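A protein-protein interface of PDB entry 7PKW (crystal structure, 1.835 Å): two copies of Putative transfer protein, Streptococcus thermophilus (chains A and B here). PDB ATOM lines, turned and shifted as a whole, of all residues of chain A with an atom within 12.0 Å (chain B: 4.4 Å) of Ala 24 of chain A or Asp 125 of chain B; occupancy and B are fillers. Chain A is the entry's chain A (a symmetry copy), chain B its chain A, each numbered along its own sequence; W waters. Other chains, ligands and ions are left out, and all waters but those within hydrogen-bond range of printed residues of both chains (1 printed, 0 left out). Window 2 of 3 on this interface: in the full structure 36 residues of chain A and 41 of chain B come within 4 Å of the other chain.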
ATOM      1  N   ASP A  23      -6.898  30.621   0.273  1.00  0.00           N
ATOM      2  CA  ASP A  23      -7.873  29.635  -0.287  1.00  0.00           C
ATOM      3  C   ASP A  23      -7.118  28.720  -1.274  1.00  0.00           C
ATOM      4  O   ASP A  23      -6.435  27.788  -0.765  1.00  0.00           O
ATOM      5  CB  ASP A  23      -9.125  30.337  -0.835  1.00  0.00           C
ATOM      6  CG  ASP A  23     -10.279  30.405   0.161  1.00  0.00           C
ATOM      7  OD1 ASP A  23     -10.866  29.338   0.465  1.00  0.00           O
ATOM      8  OD2 ASP A  23     -10.591  31.524   0.630  1.00  0.00           O
ATOM      9  N   ALA A  24      -7.188  28.969  -2.596  1.00  0.00           N
ATOM     10  CA  ALA A  24      -6.718  28.030  -3.656  1.00  0.00           C
ATOM     11  C   ALA A  24      -5.220  27.720  -3.507  1.00  0.00           C
ATOM     12  O   ALA A  24      -4.818  26.666  -4.012  1.00  0.00           O
ATOM     13  CB  ALA A  24      -6.980  28.579  -5.032  1.00  0.00           C
ATOM     14  N   ASN A  25      -4.426  28.603  -2.865  1.00  0.00           N
ATOM     15  CA  ASN A  25      -2.957  28.439  -2.645  1.00  0.00           C
ATOM     16  C   ASN A  25      -2.657  27.633  -1.371  1.00  0.00           C
ATOM     17  O   ASN A  25      -1.470  27.530  -1.032  1.00  0.00           O
ATOM     18  CB  ASN A  25      -2.234  29.789  -2.513  1.00  0.00           C
ATOM     19  CG  ASN A  25      -2.433  30.653  -3.743  1.00  0.00           C
ATOM     20  OD1 ASN A  25      -1.858  30.369  -4.792  1.00  0.00           O
ATOM     21  ND2 ASN A  25      -3.280  31.665  -3.629  1.00  0.00           N
ATOM     22  N   ARG A  26      -3.657  27.098  -0.662  1.00  0.00           N
ATOM     23  CA  ARG A  26      -3.363  26.252   0.527  1.00  0.00           C
ATOM     24  C   ARG A  26      -2.445  25.112   0.060  1.00  0.00           C
ATOM     25  O   ARG A  26      -2.496  24.771  -1.146  1.00  0.00           O
ATOM     26  CB  ARG A  26      -4.649  25.764   1.202  1.00  0.00           C
ATOM     27  CG  ARG A  26      -4.427  25.110   2.565  1.00  0.00           C
ATOM     28  CD  ARG A  26      -5.587  25.255   3.552  1.00  0.00           C
ATOM     29  NE  ARG A  26      -5.289  24.602   4.831  1.00  0.00           N
ATOM     30  CZ  ARG A  26      -6.084  23.734   5.472  1.00  0.00           C
ATOM     31  NH1 ARG A  26      -7.275  23.406   4.992  1.00  0.00           N
ATOM     32  NH2 ARG A  26      -5.686  23.190   6.611  1.00  0.00           N
ATOM     33  N   LYS A  27      -1.583  24.619   0.959  1.00  0.00           N
ATOM     34  CA  LYS A  27      -0.631  23.502   0.737  1.00  0.00           C
ATOM     35  C   LYS A  27      -1.151  22.313   1.544  1.00  0.00           C
ATOM     36  O   LYS A  27      -1.556  22.513   2.686  1.00  0.00           O
ATOM     37  CB  LYS A  27       0.790  23.881   1.149  1.00  0.00           C
ATOM     38  CG  LYS A  27       1.530  24.805   0.180  1.00  0.00           C
ATOM     39  CD  LYS A  27       1.314  26.317   0.394  1.00  0.00           C
ATOM     40  CE  LYS A  27       1.800  27.194  -0.757  1.00  0.00           C
ATOM     41  NZ  LYS A  27       1.014  26.977  -2.012  1.00  0.00           N
ATOM     42  N   TYR A  28      -1.182  21.131   0.935  1.00  0.00           N
ATOM     43  CA  TYR A  28      -1.522  19.855   1.603  1.00  0.00           C
ATOM     44  C   TYR A  28      -0.397  18.890   1.232  1.00  0.00           C
ATOM     45  O   TYR A  28       0.087  18.905   0.068  1.00  0.00           O
ATOM     46  CB  TYR A  28      -2.880  19.322   1.130  1.00  0.00           C
ATOM     47  CG  TYR A  28      -4.074  20.175   1.530  1.00  0.00           C
ATOM     48  CD1 TYR A  28      -4.562  20.180   2.824  1.00  0.00           C
ATOM     49  CD2 TYR A  28      -4.730  20.968   0.613  1.00  0.00           C
ATOM     50  CE1 TYR A  28      -5.638  20.969   3.200  1.00  0.00           C
ATOM     51  CE2 TYR A  28      -5.821  21.746   0.960  1.00  0.00           C
ATOM     52  CZ  TYR A  28      -6.280  21.752   2.258  1.00  0.00           C
ATOM     53  OH  TYR A  28      -7.361  22.530   2.583  1.00  0.00           O
ATOM     54  N   ASP A  29       0.033  18.077   2.185  1.00  0.00           N
ATOM     55  CA  ASP A  29       1.006  17.002   1.929  1.00  0.00           C
ATOM     56  C   ASP A  29       0.456  15.740   2.620  1.00  0.00           C
ATOM     57  O   ASP A  29       0.352  15.738   3.861  1.00  0.00           O
ATOM     58  CB  ASP A  29       2.382  17.439   2.404  1.00  0.00           C
ATOM     59  CG  ASP A  29       3.452  16.359   2.322  1.00  0.00           C
ATOM     60  OD1 ASP A  29       3.123  15.174   2.109  1.00  0.00           O
ATOM     61  OD2 ASP A  29       4.604  16.717   2.529  1.00  0.00           O
ATOM     62  N   TYR A  30       0.065  14.724   1.855  1.00  0.00           N
ATOM     63  CA  TYR A  30      -0.517  13.483   2.421  1.00  0.00           C
ATOM     64  C   TYR A  30       0.417  12.294   2.144  1.00  0.00           C
ATOM     65  O   TYR A  30      -0.059  11.135   2.134  1.00  0.00           O
ATOM     66  CB  TYR A  30      -1.884  13.260   1.802  1.00  0.00           C
ATOM     67  CG  TYR A  30      -2.894  14.339   2.092  1.00  0.00           C
ATOM     68  CD1 TYR A  30      -3.192  14.690   3.407  1.00  0.00           C
ATOM     69  CD2 TYR A  30      -3.612  14.958   1.083  1.00  0.00           C
ATOM     70  CE1 TYR A  30      -4.155  15.645   3.713  1.00  0.00           C
ATOM     71  CE2 TYR A  30      -4.586  15.918   1.378  1.00  0.00           C
ATOM     72  CZ  TYR A  30      -4.872  16.243   2.694  1.00  0.00           C
ATOM     73  OH  TYR A  30      -5.844  17.155   3.008  1.00  0.00           O
ATOM     74  N   LYS B  93      -1.523  25.812  -6.525  1.00  0.00           N
ATOM     75  CA  LYS B  93      -2.676  25.596  -7.451  1.00  0.00           C
ATOM     76  C   LYS B  93      -2.445  24.387  -8.362  1.00  0.00           C
ATOM     77  O   LYS B  93      -3.024  24.341  -9.482  1.00  0.00           O
ATOM     78  CB  LYS B  93      -2.939  26.847  -8.289  1.00  0.00           C
ATOM     79  CG  LYS B  93      -3.343  28.038  -7.439  1.00  0.00           C
ATOM     80  CD  LYS B  93      -3.799  29.206  -8.249  1.00  0.00           C
ATOM     81  CE  LYS B  93      -3.895  30.456  -7.403  1.00  0.00           C
ATOM     82  NZ  LYS B  93      -4.375  31.596  -8.224  1.00  0.00           N
ATOM     83  N   PHE B 124      -5.672  23.969 -10.971  1.00  0.00           N
ATOM     84  CA  PHE B 124      -7.039  24.326 -10.537  1.00  0.00           C
ATOM     85  C   PHE B 124      -7.008  25.694  -9.883  1.00  0.00           C
ATOM     86  O   PHE B 124      -5.924  26.327  -9.633  1.00  0.00           O
ATOM     87  CB  PHE B 124      -7.552  23.269  -9.544  1.00  0.00           C
ATOM     88  CG  PHE B 124      -6.885  23.359  -8.192  1.00  0.00           C
ATOM     89  CD1 PHE B 124      -5.721  22.677  -7.931  1.00  0.00           C
ATOM     90  CD2 PHE B 124      -7.409  24.148  -7.185  1.00  0.00           C
ATOM     91  CE1 PHE B 124      -5.090  22.765  -6.708  1.00  0.00           C
ATOM     92  CE2 PHE B 124      -6.755  24.269  -5.970  1.00  0.00           C
ATOM     93  CZ  PHE B 124      -5.601  23.568  -5.730  1.00  0.00           C
ATOM     94  N   ASP B 125      -8.206  26.193  -9.642  1.00  0.00           N
ATOM     95  CA  ASP B 125      -8.347  27.467  -8.920  1.00  0.00           C
ATOM     96  C   ASP B 125      -9.719  27.511  -8.254  1.00  0.00           C
ATOM     97  O   ASP B 125     -10.525  26.528  -8.330  1.00  0.00           O
ATOM     98  CB  ASP B 125      -8.112  28.651  -9.864  1.00  0.00           C
ATOM     99  CG  ASP B 125      -7.429  29.845  -9.200  1.00  0.00           C
ATOM    100  OD1 ASP B 125      -7.541  30.010  -7.950  1.00  0.00           O
ATOM    101  OD2 ASP B 125      -6.791  30.594  -9.931  1.00  0.00           O
ATOM    102  N   GLU B 126      -9.981  28.622  -7.573  1.00  0.00           N
ATOM    103  CA  GLU B 126     -11.164  28.806  -6.699  1.00  0.00           C
ATOM    104  C   GLU B 126     -11.746  30.179  -7.044  1.00  0.00           C
ATOM    105  O   GLU B 126     -10.948  31.120  -7.176  1.00  0.00           O
ATOM    106  CB  GLU B 126     -10.758  28.686  -5.221  1.00  0.00           C
ATOM    107  CG  GLU B 126     -11.918  28.439  -4.257  1.00  0.00           C
ATOM    108  CD  GLU B 126     -11.582  28.284  -2.769  1.00  0.00           C
ATOM    109  OE1 GLU B 126     -10.409  28.037  -2.455  1.00  0.00           O
ATOM    110  OE2 GLU B 126     -12.512  28.411  -1.911  1.00  0.00           O
ATOM    111  N   LYS B 130     -15.941  28.206  -4.823  1.00  0.00           N
ATOM    112  CA  LYS B 130     -16.138  27.039  -5.719  1.00  0.00           C
ATOM    113  C   LYS B 130     -14.835  26.756  -6.494  1.00  0.00           C
ATOM    114  O   LYS B 130     -14.022  27.588  -6.581  1.00  0.00           O
ATOM    115  CB  LYS B 130     -17.335  27.272  -6.647  1.00  0.00           C
ATOM    116  CG  LYS B 130     -18.707  27.179  -5.973  1.00  0.00           C
ATOM    117  CD  LYS B 130     -19.734  27.948  -6.772  1.00  0.00           C
ATOM    118  CE  LYS B 130     -21.037  28.206  -6.039  1.00  0.00           C
ATOM    119  NZ  LYS B 130     -21.626  26.939  -5.569  1.00  0.00           N
ATOM    120  N   TYR B 131     -14.746  25.618  -7.134  1.00  0.00           N
ATOM    121  CA  TYR B 131     -13.475  25.140  -7.730  1.00  0.00           C
ATOM    122  C   TYR B 131     -13.665  24.898  -9.214  1.00  0.00           C
ATOM    123  O   TYR B 131     -14.765  24.607  -9.663  1.00  0.00           O
ATOM    124  CB  TYR B 131     -13.012  23.868  -7.029  1.00  0.00           C
ATOM    125  CG  TYR B 131     -12.803  24.104  -5.560  1.00  0.00           C
ATOM    126  CD1 TYR B 131     -11.851  24.995  -5.138  1.00  0.00           C
ATOM    127  CD2 TYR B 131     -13.608  23.502  -4.601  1.00  0.00           C
ATOM    128  CE1 TYR B 131     -11.645  25.257  -3.792  1.00  0.00           C
ATOM    129  CE2 TYR B 131     -13.458  23.804  -3.249  1.00  0.00           C
ATOM    130  CZ  TYR B 131     -12.469  24.680  -2.847  1.00  0.00           C
ATOM    131  OH  TYR B 131     -12.212  24.951  -1.531  1.00  0.00           O
ATOM    132  N   TYR B 132     -12.551  24.932  -9.943  1.00  0.00           N
ATOM    133  CA  TYR B 132     -12.533  24.496 -11.358  1.00  0.00           C
ATOM    134  C   TYR B 132     -11.118  24.045 -11.730  1.00  0.00           C
ATOM    135  O   TYR B 132     -10.152  24.482 -11.106  1.00  0.00           O
ATOM    136  CB  TYR B 132     -12.932  25.639 -12.283  1.00  0.00           C
ATOM    137  CG  TYR B 132     -12.112  26.909 -12.217  1.00  0.00           C
ATOM    138  CD1 TYR B 132     -12.321  27.865 -11.242  1.00  0.00           C
ATOM    139  CD2 TYR B 132     -11.169  27.214 -13.200  1.00  0.00           C
ATOM    140  CE1 TYR B 132     -11.619  29.069 -11.232  1.00  0.00           C
ATOM    141  CE2 TYR B 132     -10.427  28.390 -13.165  1.00  0.00           C
ATOM    142  CZ  TYR B 132     -10.677  29.337 -12.202  1.00  0.00           C
ATOM    143  OH  TYR B 132      -9.958  30.505 -12.132  1.00  0.00           O
HETATM  144  O   HOH W   1      -2.566  25.282  -4.055  1.00  0.00           O
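Water W1 lies within hydrogen-bond range of the backbone carbonyl oxygen (O) of Ala 24 of chain A, the backbone NH (N) of Lys 93 of chain B and the backbone carbonyl oxygen (O) of Arg 26 of chain A.
The backbone carbonyl oxygen of Lys 93 of chain B lies within hydrogen-bond range of the backbone NH of Phe 124 of chain B (3.1 Å). The side-chain amino group (NZ) of Lys 93 of chain B lies within salt-bridge range of the side-chain carboxylate (OD2) of Asp 125 of chain B, 3.1 Å away. The backbone carbonyl oxygen (O) of Tyr 132 of chain B lies within hydrogen-bond range of the backbone NH (N) of Asp 125 of chain B (3.0 Å). OH of Tyr 131 of chain B is in hydrogen-bond range of OE2 of Glu 126 of chain B (3.5 Å). The side-chain amino group (NZ) of Lys 27 of chain A lies within hydrogen-bond range of the backbone carbonyl oxygen (O) of Asn 25 of chain A, at 2.7 Å.
Printed residues of chain B that touch a printed residue of chain A: Lys 93, Phe 124, Asp 125 and Glu 126. Hydrophobic or aromatic side chains of chain B that line the printed part of chain A: Phe 124. Along chain B the printed residues that touch a printed residue of chain A span positions 93 to 126.
Among the printed residues, pairs that only touch across the chains: Ala 24 of chain A with Lys 93 of chain B, Ala 24 of chain A with Phe 124 of chain B, Ala 24 of chain A with Asp 125 of chain B and Asn 25 of chain A with Lys 93 of chain B.
OE1 of Glu 126 of chain B sits at hydrogen-bond distance from N of Ala 24 of chain A, at 3.4 Å. The side-chain carboxylate (OD1) of Asp 23 of chain A sits close to the side-chain carboxylate (OE2) of Glu 126 of chain B, at 3.0 Å.
Printed residues of chain B within 4 Å of Asp 23 of chain A: Glu 126. Printed residues of chain B within 4 Å of Ala 24 of chain A: Lys 93 (3.98 Å), Phe 124 (3.6 Å), Asp 125 (3.3 Å) and Glu 126 (3.4 Å). Of the printed residues of chain B, Asn 25 of chain A touches Lys 93 (3.3 Å). Lys 93 of chain B touches just these residues of chain A: Ala 24 and Asn 25. Of the printed residues of chain A, Asp 125 of chain B touches Ala 24. Printed residues of chain A within 4 Å of Glu 126 of chain B: Asp 23 and Ala 24. No residue of chain A comes within 4 Å of Tyr 132 of chain B. The nearest residue of chain A that does not touch Asp 125 of chain B is Asn 25 of chain A (6.1 Å).
No position is printed for both chains. Of the 6 pairs that touch across the chains among the printed residues, none has its exchanged pair printed and touching as well.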
